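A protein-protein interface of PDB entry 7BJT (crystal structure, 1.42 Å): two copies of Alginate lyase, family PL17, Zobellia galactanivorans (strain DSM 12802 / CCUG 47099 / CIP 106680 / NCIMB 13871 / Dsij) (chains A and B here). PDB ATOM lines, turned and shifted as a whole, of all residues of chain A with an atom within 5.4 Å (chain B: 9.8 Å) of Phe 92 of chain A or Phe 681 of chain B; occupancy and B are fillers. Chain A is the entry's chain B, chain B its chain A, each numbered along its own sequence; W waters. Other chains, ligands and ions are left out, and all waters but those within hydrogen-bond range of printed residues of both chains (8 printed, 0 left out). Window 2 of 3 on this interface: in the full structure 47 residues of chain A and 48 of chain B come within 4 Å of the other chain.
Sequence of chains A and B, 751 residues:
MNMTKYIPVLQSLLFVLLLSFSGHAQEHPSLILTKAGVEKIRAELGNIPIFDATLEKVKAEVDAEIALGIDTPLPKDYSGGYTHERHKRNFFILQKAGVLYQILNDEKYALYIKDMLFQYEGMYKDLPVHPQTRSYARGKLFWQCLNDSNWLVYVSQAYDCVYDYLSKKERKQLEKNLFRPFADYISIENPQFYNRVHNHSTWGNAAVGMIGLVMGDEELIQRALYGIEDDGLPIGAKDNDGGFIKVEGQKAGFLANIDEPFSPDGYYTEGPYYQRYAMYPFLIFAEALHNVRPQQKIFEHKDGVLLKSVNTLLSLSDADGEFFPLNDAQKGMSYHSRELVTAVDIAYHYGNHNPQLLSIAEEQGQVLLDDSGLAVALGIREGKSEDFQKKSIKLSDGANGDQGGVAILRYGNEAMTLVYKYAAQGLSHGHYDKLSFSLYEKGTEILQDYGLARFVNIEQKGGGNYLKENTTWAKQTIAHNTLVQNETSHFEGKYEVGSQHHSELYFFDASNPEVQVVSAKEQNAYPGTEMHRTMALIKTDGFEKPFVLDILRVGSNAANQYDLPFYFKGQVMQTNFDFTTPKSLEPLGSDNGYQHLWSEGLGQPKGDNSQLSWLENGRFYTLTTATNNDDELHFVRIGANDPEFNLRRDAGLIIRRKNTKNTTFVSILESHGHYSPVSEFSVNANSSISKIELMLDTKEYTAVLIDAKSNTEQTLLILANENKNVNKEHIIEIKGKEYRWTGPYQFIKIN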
ATOM      1  N   GLU A  85      22.254  20.049  10.352  1.00  0.00           N
ATOM      2  CA  GLU A  85      22.225  19.699  11.761  1.00  0.00           C
ATOM      3  C   GLU A  85      22.970  20.704  12.633  1.00  0.00           C
ATOM      4  O   GLU A  85      22.548  20.965  13.757  1.00  0.00           O
ATOM      5  CB  GLU A  85      22.755  18.278  11.991  1.00  0.00           C
ATOM      6  CG  GLU A  85      21.921  17.191  11.315  1.00  0.00           C
ATOM      7  CD  GLU A  85      20.454  17.219  11.704  1.00  0.00           C
ATOM      8  OE1 GLU A  85      20.133  17.246  12.916  1.00  0.00           O
ATOM      9  OE2 GLU A  85      19.594  17.232  10.800  1.00  0.00           O
ATOM     10  N   LYS A  88      20.837  23.925  12.814  1.00  0.00           N
ATOM     11  CA  LYS A  88      19.667  23.560  13.618  1.00  0.00           C
ATOM     12  C   LYS A  88      20.010  23.488  15.107  1.00  0.00           C
ATOM     13  O   LYS A  88      19.335  24.106  15.948  1.00  0.00           O
ATOM     14  CB  LYS A  88      19.070  22.241  13.126  1.00  0.00           C
ATOM     15  CG  LYS A  88      17.816  21.793  13.853  1.00  0.00           C
ATOM     16  CD  LYS A  88      17.139  20.668  13.081  1.00  0.00           C
ATOM     17  CE  LYS A  88      15.920  20.122  13.799  1.00  0.00           C
ATOM     18  NZ  LYS A  88      15.279  19.032  13.005  1.00  0.00           N
ATOM     19  N   ARG A  89      21.079  22.770  15.440  1.00  0.00           N
ATOM     20  CA  ARG A  89      21.519  22.701  16.834  1.00  0.00           C
ATOM     21  C   ARG A  89      21.842  24.096  17.374  1.00  0.00           C
ATOM     22  O   ARG A  89      21.533  24.399  18.526  1.00  0.00           O
ATOM     23  CB  ARG A  89      22.719  21.768  17.007  1.00  0.00           C
ATOM     24  CG  ARG A  89      23.075  21.568  18.478  1.00  0.00           C
ATOM     25  CD  ARG A  89      24.125  20.511  18.719  1.00  0.00           C
ATOM     26  NE  ARG A  89      23.635  19.159  18.451  1.00  0.00           N
ATOM     27  CZ  ARG A  89      24.224  18.041  18.875  1.00  0.00           C
ATOM     28  NH1 ARG A  89      23.691  16.861  18.567  1.00  0.00           N
ATOM     29  NH2 ARG A  89      25.344  18.084  19.605  1.00  0.00           N
ATOM     30  N   ASN A  90      22.457  24.939  16.548  1.00  0.00           N
ATOM     31  CA  ASN A  90      22.763  26.300  16.979  1.00  0.00           C
ATOM     32  C   ASN A  90      21.532  27.073  17.440  1.00  0.00           C
ATOM     33  O   ASN A  90      21.599  27.748  18.457  1.00  0.00           O
ATOM     34  CB  ASN A  90      23.472  27.102  15.887  1.00  0.00           C
ATOM     35  CG  ASN A  90      24.918  26.691  15.676  1.00  0.00           C
ATOM     36  OD1 ASN A  90      25.510  25.938  16.461  1.00  0.00           O
ATOM     37  ND2 ASN A  90      25.504  27.205  14.604  1.00  0.00           N
ATOM     38  N   PHE A  91      20.414  26.991  16.716  1.00  0.00           N
ATOM     39  CA  PHE A  91      19.232  27.735  17.162  1.00  0.00           C
ATOM     40  C   PHE A  91      18.643  27.192  18.461  1.00  0.00           C
ATOM     41  O   PHE A  91      18.235  27.971  19.330  1.00  0.00           O
ATOM     42  CB  PHE A  91      18.191  28.024  16.044  1.00  0.00           C
ATOM     43  CG  PHE A  91      17.348  26.855  15.567  1.00  0.00           C
ATOM     44  CD1 PHE A  91      16.386  26.251  16.382  1.00  0.00           C
ATOM     45  CD2 PHE A  91      17.409  26.467  14.234  1.00  0.00           C
ATOM     46  CE1 PHE A  91      15.578  25.235  15.895  1.00  0.00           C
ATOM     47  CE2 PHE A  91      16.590  25.466  13.738  1.00  0.00           C
ATOM     48  CZ  PHE A  91      15.676  24.845  14.572  1.00  0.00           C
ATOM     49  N   PHE A  92      18.659  25.872  18.636  1.00  0.00           N
ATOM     50  CA  PHE A  92      18.215  25.287  19.905  1.00  0.00           C
ATOM     51  C   PHE A  92      19.113  25.724  21.059  1.00  0.00           C
ATOM     52  O   PHE A  92      18.629  26.089  22.131  1.00  0.00           O
ATOM     53  CB  PHE A  92      18.181  23.753  19.838  1.00  0.00           C
ATOM     54  CG  PHE A  92      17.040  23.191  19.029  1.00  0.00           C
ATOM     55  CD1 PHE A  92      15.717  23.492  19.349  1.00  0.00           C
ATOM     56  CD2 PHE A  92      17.278  22.319  17.970  1.00  0.00           C
ATOM     57  CE1 PHE A  92      14.663  22.954  18.621  1.00  0.00           C
ATOM     58  CE2 PHE A  92      16.223  21.782  17.243  1.00  0.00           C
ATOM     59  CZ  PHE A  92      14.916  22.105  17.566  1.00  0.00           C
ATOM     60  N   ILE A  93      20.421  25.692  20.836  1.00  0.00           N
ATOM     61  CA  ILE A  93      21.378  26.054  21.882  1.00  0.00           C
ATOM     62  C   ILE A  93      21.296  27.541  22.236  1.00  0.00           C
ATOM     63  O   ILE A  93      21.405  27.894  23.410  1.00  0.00           O
ATOM     64  CB  ILE A  93      22.813  25.632  21.486  1.00  0.00           C
ATOM     65  CG1 ILE A  93      22.913  24.095  21.471  1.00  0.00           C
ATOM     66  CG2 ILE A  93      23.874  26.235  22.408  1.00  0.00           C
ATOM     67  CD1 ILE A  93      22.875  23.411  22.828  1.00  0.00           C
ATOM     68  N   LEU A  94      21.093  28.401  21.240  1.00  0.00           N
ATOM     69  CA  LEU A  94      20.981  29.834  21.509  1.00  0.00           C
ATOM     70  C   LEU A  94      19.797  30.143  22.425  1.00  0.00           C
ATOM     71  O   LEU A  94      19.947  30.877  23.393  1.00  0.00           O
ATOM     72  CB  LEU A  94      20.887  30.644  20.210  1.00  0.00           C
ATOM     73  CG  LEU A  94      22.220  30.853  19.481  1.00  0.00           C
ATOM     74  CD1 LEU A  94      22.008  31.293  18.041  1.00  0.00           C
ATOM     75  CD2 LEU A  94      23.094  31.867  20.204  1.00  0.00           C
ATOM     76  N   GLN A  95      18.629  29.561  22.151  1.00  0.00           N
ATOM     77  CA  GLN A  95      17.462  29.793  23.009  1.00  0.00           C
ATOM     78  C   GLN A  95      17.717  29.265  24.427  1.00  0.00           C
ATOM     79  O   GLN A  95      17.362  29.908  25.409  1.00  0.00           O
ATOM     80  CB  GLN A  95      16.201  29.182  22.381  1.00  0.00           C
ATOM     81  CG  GLN A  95      14.909  29.438  23.158  1.00  0.00           C
ATOM     82  CD  GLN A  95      14.731  28.547  24.382  1.00  0.00           C
ATOM     83  OE1 GLN A  95      15.138  27.383  24.392  1.00  0.00           O
ATOM     84  NE2 GLN A  95      14.105  29.085  25.419  1.00  0.00           N
ATOM     85  N   LYS A  96      18.347  28.101  24.530  1.00  0.00           N
ATOM     86  CA  LYS A  96      18.693  27.546  25.839  1.00  0.00           C
ATOM     87  C   LYS A  96      19.664  28.447  26.599  1.00  0.00           C
ATOM     88  O   LYS A  96      19.458  28.727  27.772  1.00  0.00           O
ATOM     89  CB  LYS A  96      19.253  26.136  25.693  1.00  0.00           C
ATOM     90  CG  LYS A  96      18.167  25.135  25.357  1.00  0.00           C
ATOM     91  CD  LYS A  96      18.732  23.792  24.941  1.00  0.00           C
ATOM     92  CE  LYS A  96      17.599  22.843  24.610  1.00  0.00           C
ATOM     93  NZ  LYS A  96      18.118  21.520  24.209  1.00  0.00           N
ATOM     94  N   ALA A  97      20.706  28.908  25.917  1.00  0.00           N
ATOM     95  CA  ALA A  97      21.677  29.815  26.529  1.00  0.00           C
ATOM     96  C   ALA A  97      21.018  31.096  27.030  1.00  0.00           C
ATOM     97  O   ALA A  97      21.402  31.620  28.070  1.00  0.00           O
ATOM     98  CB  ALA A  97      22.791  30.140  25.552  1.00  0.00           C
ATOM     99  N   TYR A 154      13.514  30.735  17.253  1.00  0.00           N
ATOM    100  CA  TYR A 154      14.327  30.388  18.420  1.00  0.00           C
ATOM    101  C   TYR A 154      15.346  31.476  18.758  1.00  0.00           C
ATOM    102  O   TYR A 154      15.515  31.825  19.930  1.00  0.00           O
ATOM    103  CB  TYR A 154      15.018  29.029  18.217  1.00  0.00           C
ATOM    104  CG  TYR A 154      14.114  27.851  18.509  1.00  0.00           C
ATOM    105  CD1 TYR A 154      13.232  27.359  17.549  1.00  0.00           C
ATOM    106  CD2 TYR A 154      14.147  27.225  19.746  1.00  0.00           C
ATOM    107  CE1 TYR A 154      12.409  26.279  17.821  1.00  0.00           C
ATOM    108  CE2 TYR A 154      13.330  26.143  20.030  1.00  0.00           C
ATOM    109  CZ  TYR A 154      12.470  25.673  19.063  1.00  0.00           C
ATOM    110  OH  TYR A 154      11.660  24.592  19.355  1.00  0.00           O
ATOM    111  N   ARG A 338       9.290  18.152  21.956  1.00  0.00           N
ATOM    112  CA  ARG A 338       9.526  19.519  22.440  1.00  0.00           C
ATOM    113  C   ARG A 338       8.331  20.436  22.179  1.00  0.00           C
ATOM    114  O   ARG A 338       8.024  21.311  22.993  1.00  0.00           O
ATOM    115  CB  ARG A 338      10.801  20.115  21.836  1.00  0.00           C
ATOM    116  CG  ARG A 338      10.760  20.368  20.335  1.00  0.00           C
ATOM    117  CD  ARG A 338      12.121  20.799  19.808  1.00  0.00           C
ATOM    118  NE  ARG A 338      13.055  19.686  19.755  1.00  0.00           N
ATOM    119  CZ  ARG A 338      13.272  18.889  18.702  1.00  0.00           C
ATOM    120  NH1 ARG A 338      12.639  19.062  17.547  1.00  0.00           N
ATOM    121  NH2 ARG A 338      14.155  17.903  18.811  1.00  0.00           N
ATOM    122  N   ASN A 457      14.273  13.552   8.475  1.00  0.00           N
ATOM    123  CA  ASN A 457      15.606  14.050   8.817  1.00  0.00           C
ATOM    124  C   ASN A 457      16.718  12.993   8.790  1.00  0.00           C
ATOM    125  O   ASN A 457      17.805  13.230   9.327  1.00  0.00           O
ATOM    126  CB  ASN A 457      15.621  14.813  10.161  1.00  0.00           C
ATOM    127  CG  ASN A 457      14.636  15.970  10.209  1.00  0.00           C
ATOM    128  OD1 ASN A 457      14.420  16.670   9.212  1.00  0.00           O
ATOM    129  ND2 ASN A 457      14.055  16.198  11.376  1.00  0.00           N
ATOM    130  N   LEU B 615      18.628   0.530  10.022  1.00  0.00           N
ATOM    131  CA  LEU B 615      18.182   1.150  11.261  1.00  0.00           C
ATOM    132  C   LEU B 615      17.308   0.140  11.992  1.00  0.00           C
ATOM    133  O   LEU B 615      16.330  -0.356  11.423  1.00  0.00           O
ATOM    134  CB  LEU B 615      17.372   2.409  10.943  1.00  0.00           C
ATOM    135  CG  LEU B 615      16.658   3.121  12.093  1.00  0.00           C
ATOM    136  CD1 LEU B 615      17.636   3.668  13.109  1.00  0.00           C
ATOM    137  CD2 LEU B 615      15.774   4.233  11.552  1.00  0.00           C
ATOM    138  N   GLY B 618      16.128   2.189  16.807  1.00  0.00           N
ATOM    139  CA  GLY B 618      16.726   3.486  17.060  1.00  0.00           C
ATOM    140  C   GLY B 618      18.235   3.571  16.939  1.00  0.00           C
ATOM    141  O   GLY B 618      18.798   4.598  17.304  1.00  0.00           O
ATOM    142  N   ARG B 619      18.888   2.540  16.404  1.00  0.00           N
ATOM    143  CA  ARG B 619      20.344   2.521  16.239  1.00  0.00           C
ATOM    144  C   ARG B 619      20.672   2.157  14.794  1.00  0.00           C
ATOM    145  O   ARG B 619      19.955   1.356  14.174  1.00  0.00           O
ATOM    146  CB  ARG B 619      20.980   1.508  17.182  1.00  0.00           C
ATOM    147  CG  ARG B 619      20.694   1.750  18.654  1.00  0.00           C
ATOM    148  CD  ARG B 619      21.530   0.813  19.510  1.00  0.00           C
ATOM    149  NE  ARG B 619      21.265   0.929  20.947  1.00  0.00           N
ATOM    150  CZ  ARG B 619      20.389   0.200  21.645  1.00  0.00           C
ATOM    151  NH1 ARG B 619      19.633  -0.739  21.075  1.00  0.00           N
ATOM    152  NH2 ARG B 619      20.278   0.404  22.957  1.00  0.00           N
ATOM    153  N   PHE B 620      21.753   2.724  14.251  1.00  0.00           N
ATOM    154  CA  PHE B 620      22.228   2.341  12.919  1.00  0.00           C
ATOM    155  C   PHE B 620      23.287   1.249  12.998  1.00  0.00           C
ATOM    156  O   PHE B 620      24.043   1.152  13.980  1.00  0.00           O
ATOM    157  CB  PHE B 620      22.774   3.538  12.124  1.00  0.00           C
ATOM    158  CG  PHE B 620      21.774   4.640  11.905  1.00  0.00           C
ATOM    159  CD1 PHE B 620      20.838   4.572  10.872  1.00  0.00           C
ATOM    160  CD2 PHE B 620      21.782   5.766  12.719  1.00  0.00           C
ATOM    161  CE1 PHE B 620      19.934   5.602  10.665  1.00  0.00           C
ATOM    162  CE2 PHE B 620      20.872   6.795  12.518  1.00  0.00           C
ATOM    163  CZ  PHE B 620      19.952   6.710  11.492  1.00  0.00           C
ATOM    164  N   GLY B 673      25.588   5.528  16.164  1.00  0.00           N
ATOM    165  CA  GLY B 673      24.585   6.564  16.130  1.00  0.00           C
ATOM    166  C   GLY B 673      23.215   6.152  16.603  1.00  0.00           C
ATOM    167  O   GLY B 673      23.032   5.093  17.200  1.00  0.00           O
ATOM    168  N   HIS B 674      22.252   7.020  16.323  1.00  0.00           N
ATOM    169  CA  HIS B 674      20.890   6.809  16.785  1.00  0.00           C
ATOM    170  C   HIS B 674      19.907   7.698  16.066  1.00  0.00           C
ATOM    171  O   HIS B 674      20.281   8.706  15.467  1.00  0.00           O
ATOM    172  CB  HIS B 674      20.776   7.023  18.301  1.00  0.00           C
ATOM    173  CG  HIS B 674      21.459   8.254  18.796  1.00  0.00           C
ATOM    174  ND1 HIS B 674      20.842   9.484  18.837  1.00  0.00           N
ATOM    175  CD2 HIS B 674      22.710   8.443  19.285  1.00  0.00           C
ATOM    176  CE1 HIS B 674      21.682  10.379  19.333  1.00  0.00           C
ATOM    177  NE2 HIS B 674      22.824   9.773  19.605  1.00  0.00           N
ATOM    178  N   TYR B 675      18.649   7.272  16.111  1.00  0.00           N
ATOM    179  CA  TYR B 675      17.524   8.041  15.600  1.00  0.00           C
ATOM    180  C   TYR B 675      16.384   7.941  16.602  1.00  0.00           C
ATOM    181  O   TYR B 675      16.211   6.910  17.253  1.00  0.00           O
ATOM    182  CB  TYR B 675      17.058   7.519  14.242  1.00  0.00           C
ATOM    183  CG  TYR B 675      15.953   8.372  13.673  1.00  0.00           C
ATOM    184  CD1 TYR B 675      16.234   9.623  13.136  1.00  0.00           C
ATOM    185  CD2 TYR B 675      14.618   7.958  13.718  1.00  0.00           C
ATOM    186  CE1 TYR B 675      15.227  10.432  12.636  1.00  0.00           C
ATOM    187  CE2 TYR B 675      13.604   8.766  13.224  1.00  0.00           C
ATOM    188  CZ  TYR B 675      13.917   9.996  12.674  1.00  0.00           C
ATOM    189  OH  TYR B 675      12.917  10.800  12.178  1.00  0.00           O
ATOM    190  N   SER B 676      15.606   9.015  16.719  1.00  0.00           N
ATOM    191  CA  SER B 676      14.394   9.029  17.527  1.00  0.00           C
ATOM    192  C   SER B 676      13.277   9.667  16.718  1.00  0.00           C
ATOM    193  O   SER B 676      13.467  10.749  16.180  1.00  0.00           O
ATOM    194  CB  SER B 676      14.604   9.859  18.792  1.00  0.00           C
ATOM    195  OG  SER B 676      13.353  10.185  19.396  1.00  0.00           O
ATOM    196  N   PRO B 677      12.091   9.034  16.677  1.00  0.00           N
ATOM    197  CA  PRO B 677      10.951   9.695  16.050  1.00  0.00           C
ATOM    198  C   PRO B 677      10.264  10.729  16.948  1.00  0.00           C
ATOM    199  O   PRO B 677       9.247  11.289  16.553  1.00  0.00           O
ATOM    200  CB  PRO B 677      10.014   8.529  15.739  1.00  0.00           C
ATOM    201  CG  PRO B 677      10.261   7.585  16.853  1.00  0.00           C
ATOM    202  CD  PRO B 677      11.736   7.679  17.141  1.00  0.00           C
ATOM    203  N   VAL B 678      10.802  10.986  18.139  1.00  0.00           N
ATOM    204  CA  VAL B 678      10.307  12.058  19.006  1.00  0.00           C
ATOM    205  C   VAL B 678      11.111  13.332  18.765  1.00  0.00           C
ATOM    206  O   VAL B 678      10.537  14.387  18.509  1.00  0.00           O
ATOM    207  CB  VAL B 678      10.345  11.635  20.485  1.00  0.00           C
ATOM    208  CG1 VAL B 678       9.822  12.741  21.389  1.00  0.00           C
ATOM    209  CG2 VAL B 678       9.508  10.378  20.685  1.00  0.00           C
ATOM    210  N   SER B 679      12.435  13.236  18.851  1.00  0.00           N
ATOM    211  CA  SER B 679      13.308  14.376  18.554  1.00  0.00           C
ATOM    212  C   SER B 679      13.514  14.604  17.061  1.00  0.00           C
ATOM    213  O   SER B 679      13.858  15.713  16.654  1.00  0.00           O
ATOM    214  CB  SER B 679      14.667  14.180  19.207  1.00  0.00           C
ATOM    215  OG  SER B 679      15.377  13.145  18.549  1.00  0.00           O
ATOM    216  N   GLU B 680      13.355  13.539  16.272  1.00  0.00           N
ATOM    217  CA  GLU B 680      13.648  13.534  14.832  1.00  0.00           C
ATOM    218  C   GLU B 680      15.082  13.970  14.515  1.00  0.00           C
ATOM    219  O   GLU B 680      15.337  14.583  13.483  1.00  0.00           O
ATOM    220  CB  GLU B 680      12.583  14.321  14.052  1.00  0.00           C
ATOM    221  CG  GLU B 680      11.190  13.732  14.234  1.00  0.00           C
ATOM    222  CD  GLU B 680      10.127  14.371  13.365  1.00  0.00           C
ATOM    223  OE1 GLU B 680      10.161  15.594  13.159  1.00  0.00           O
ATOM    224  OE2 GLU B 680       9.246  13.627  12.892  1.00  0.00           O
ATOM    225  N   PHE B 681      16.012  13.621  15.409  1.00  0.00           N
ATOM    226  CA  PHE B 681      17.435  13.800  15.163  1.00  0.00           C
ATOM    227  C   PHE B 681      18.050  12.473  14.757  1.00  0.00           C
ATOM    228  O   PHE B 681      17.896  11.472  15.458  1.00  0.00           O
ATOM    229  CB  PHE B 681      18.192  14.267  16.414  1.00  0.00           C
ATOM    230  CG  PHE B 681      17.913  15.683  16.825  1.00  0.00           C
ATOM    231  CD1 PHE B 681      18.032  16.729  15.923  1.00  0.00           C
ATOM    232  CD2 PHE B 681      17.601  15.972  18.147  1.00  0.00           C
ATOM    233  CE1 PHE B 681      17.793  18.039  16.326  1.00  0.00           C
ATOM    234  CE2 PHE B 681      17.362  17.274  18.557  1.00  0.00           C
ATOM    235  CZ  PHE B 681      17.451  18.304  17.640  1.00  0.00           C
ATOM    236  N   SER B 682      18.759  12.496  13.635  1.00  0.00           N
ATOM    237  CA  SER B 682      19.609  11.399  13.197  1.00  0.00           C
ATOM    238  C   SER B 682      21.043  11.773  13.519  1.00  0.00           C
ATOM    239  O   SER B 682      21.507  12.828  13.088  1.00  0.00           O
ATOM    240  CB  SER B 682      19.439  11.197  11.690  1.00  0.00           C
ATOM    241  OG  SER B 682      20.186  10.086  11.241  1.00  0.00           O
ATOM    242  N   VAL B 683      21.733  10.929  14.281  1.00  0.00           N
ATOM    243  CA  VAL B 683      23.106  11.200  14.728  1.00  0.00           C
ATOM    244  C   VAL B 683      24.008  10.046  14.309  1.00  0.00           C
ATOM    245  O   VAL B 683      23.617   8.889  14.431  1.00  0.00           O
ATOM    246  CB  VAL B 683      23.154  11.397  16.257  1.00  0.00           C
ATOM    247  CG1 VAL B 683      24.588  11.553  16.752  1.00  0.00           C
ATOM    248  CG2 VAL B 683      22.321  12.616  16.653  1.00  0.00           C
ATOM    249  N   ASN B 684      25.193  10.378  13.796  1.00  0.00           N
ATOM    250  CA  ASN B 684      26.223   9.401  13.430  1.00  0.00           C
ATOM    251  C   ASN B 684      25.679   8.218  12.629  1.00  0.00           C
ATOM    252  O   ASN B 684      25.853   7.053  12.989  1.00  0.00           O
ATOM    253  CB  ASN B 684      26.995   8.947  14.677  1.00  0.00           C
ATOM    254  CG  ASN B 684      27.816  10.067  15.315  1.00  0.00           C
ATOM    255  OD1 ASN B 684      27.957  10.119  16.541  1.00  0.00           O
ATOM    256  ND2 ASN B 684      28.370  10.954  14.498  1.00  0.00           N
ATOM    257  N   ALA B 685      25.026   8.555  11.527  1.00  0.00           N
ATOM    258  CA  ALA B 685      24.328   7.592  10.683  1.00  0.00           C
ATOM    259  C   ALA B 685      25.220   6.919   9.638  1.00  0.00           C
ATOM    260  O   ALA B 685      24.770   6.000   8.963  1.00  0.00           O
ATOM    261  CB  ALA B 685      23.145   8.273   9.999  1.00  0.00           C
HETATM  262  O   HOH W   1      13.635  17.823  14.875  1.00  0.00           O
HETATM  263  O   HOH W   2      12.014  18.064  12.126  1.00  0.00           O
HETATM  264  O   HOH W   3      10.796  17.568  14.975  1.00  0.00           O
HETATM  265  O   HOH W   4      18.627  14.537  11.680  1.00  0.00           O
HETATM  266  O   HOH W   5       9.856  17.144  17.560  1.00  0.00           O
HETATM  267  O   HOH W   6      17.123  17.070  12.556  1.00  0.00           O
HETATM  268  O   HOH W   7      21.555  15.366  14.395  1.00  0.00           O
HETATM  269  O   HOH W   8      11.131  16.851  20.258  1.00  0.00           O
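The backbone carbonyl oxygen of Ser 679 of chain B is in hydrogen-bond range of the guanidinium group of Arg 338 of chain A, 3.1 Å away. The side-chain amide nitrogen (ND2) of Asn 457 of chain A lies within hydrogen-bond range of the backbone carbonyl oxygen (O) of Glu 680 of chain B (2.9 Å).
The side-chain hydroxyl (OG) of Ser 676 of chain B lies within hydrogen-bond range of the backbone NH (N) of Ser 679 of chain B (3.2 Å). The side-chain amino group of Lys 88 of chain A lies close to the side-chain amide nitrogen of Asn 457 of chain A, at 3.5 Å. OG of Ser 679 of chain B lies close to N of Phe 681 of chain B (3.2 Å).
Among the printed residues, merely in contact across the chains: Glu 85 of chain A with Phe 681 of chain B (3.7 Å), Lys 88 of chain A with Phe 681 of chain B (3.8 Å), Phe 92 of chain A with Phe 681 of chain B (3.7 Å), Arg 338 of chain A with Phe 681 of chain B (3.3 Å) and Asn 457 of chain A with Ser 682 of chain B (3.5 Å).
Printed residues of chain B within 4 Å of Lys 88 of chain A: Phe 681 (3.8 Å). No residue of chain B comes within 4 Å of Phe 91 of chain A. Phe 92 of chain A touches just one residue of chain B: Phe 681 (3.7 Å). No residue of chain B comes within 4 Å of Ile 93 of chain A. Lys 96 of chain A touches none of the printed residues of chain B. Printed residues of chain B within 4 Å of Arg 338 of chain A: Ser 679 and Phe 681. Gly 673 of chain B touches none of the printed residues of chain A. Of chain A, only Glu 85 (3.7 Å), Lys 88 (3.8 Å), Phe 92 (3.7 Å) and Arg 338 (3.3 Å) come within 4 Å of Phe 681 of chain B. The nearest residue of chain A that does not touch Phe 681 of chain B is Asn 457 of chain A (5.2 Å). The nearest printed residue of chain B that does not touch Glu 85 of chain A is Ser 682 of chain B (4.6 Å).
Hydrophobic or aromatic side chains of chain B within 4 Å of the printed part of chain A: Phe 681. Printed residues of chain A that touch a printed residue of chain B: Glu 85, Lys 88, Phe 92, Arg 338 and Asn 457. Among the printed residues, 7 pairs touch across the chains. Among the printed residues, no Asp or Glu carboxylate lies within 4 Å of a Lys or Arg side-chain nitrogen of the other chain.
No position is printed for both chains.
Water W6 lies within hydrogen-bond range of the side-chain amino group of Lys 88 of chain A (2.7 Å), the side-chain carboxylate of Glu 85 of chain A (3.0 Å), the backbone carbonyl oxygen of Glu 680 of chain B (3.2 Å) and the side-chain amide nitrogen of Asn 457 of chain A (3.4 Å). Water W1 lies within hydrogen-bond range of NZ of Lys 88 of chain A (2.8 Å), O of Ser 679 of chain B (2.8 Å) and NH1 of Arg 338 of chain A (3.1 Å). Water W7 bridges OE1 of Glu 85 of chain A and O of Ser 682 of chain B. Water W4 lies within hydrogen-bond range of the backbone carbonyl oxygen (O) of Asn 457 of chain A (2.8 Å), the backbone NH (N) of Ser 682 of chain B (2.8 Å) and the side-chain carboxylate (OE2) of Glu 85 of chain A (3.0 Å). Water W2 lies within hydrogen-bond range of ND2 of Asn 457 of chain A and OE1 of Glu 680 of chain B. Water W5 lies within hydrogen-bond range of the backbone carbonyl oxygen of Val 678 of chain B (3.0 Å) and the guanidinium group of Arg 338 of chain A (3.4 Å).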
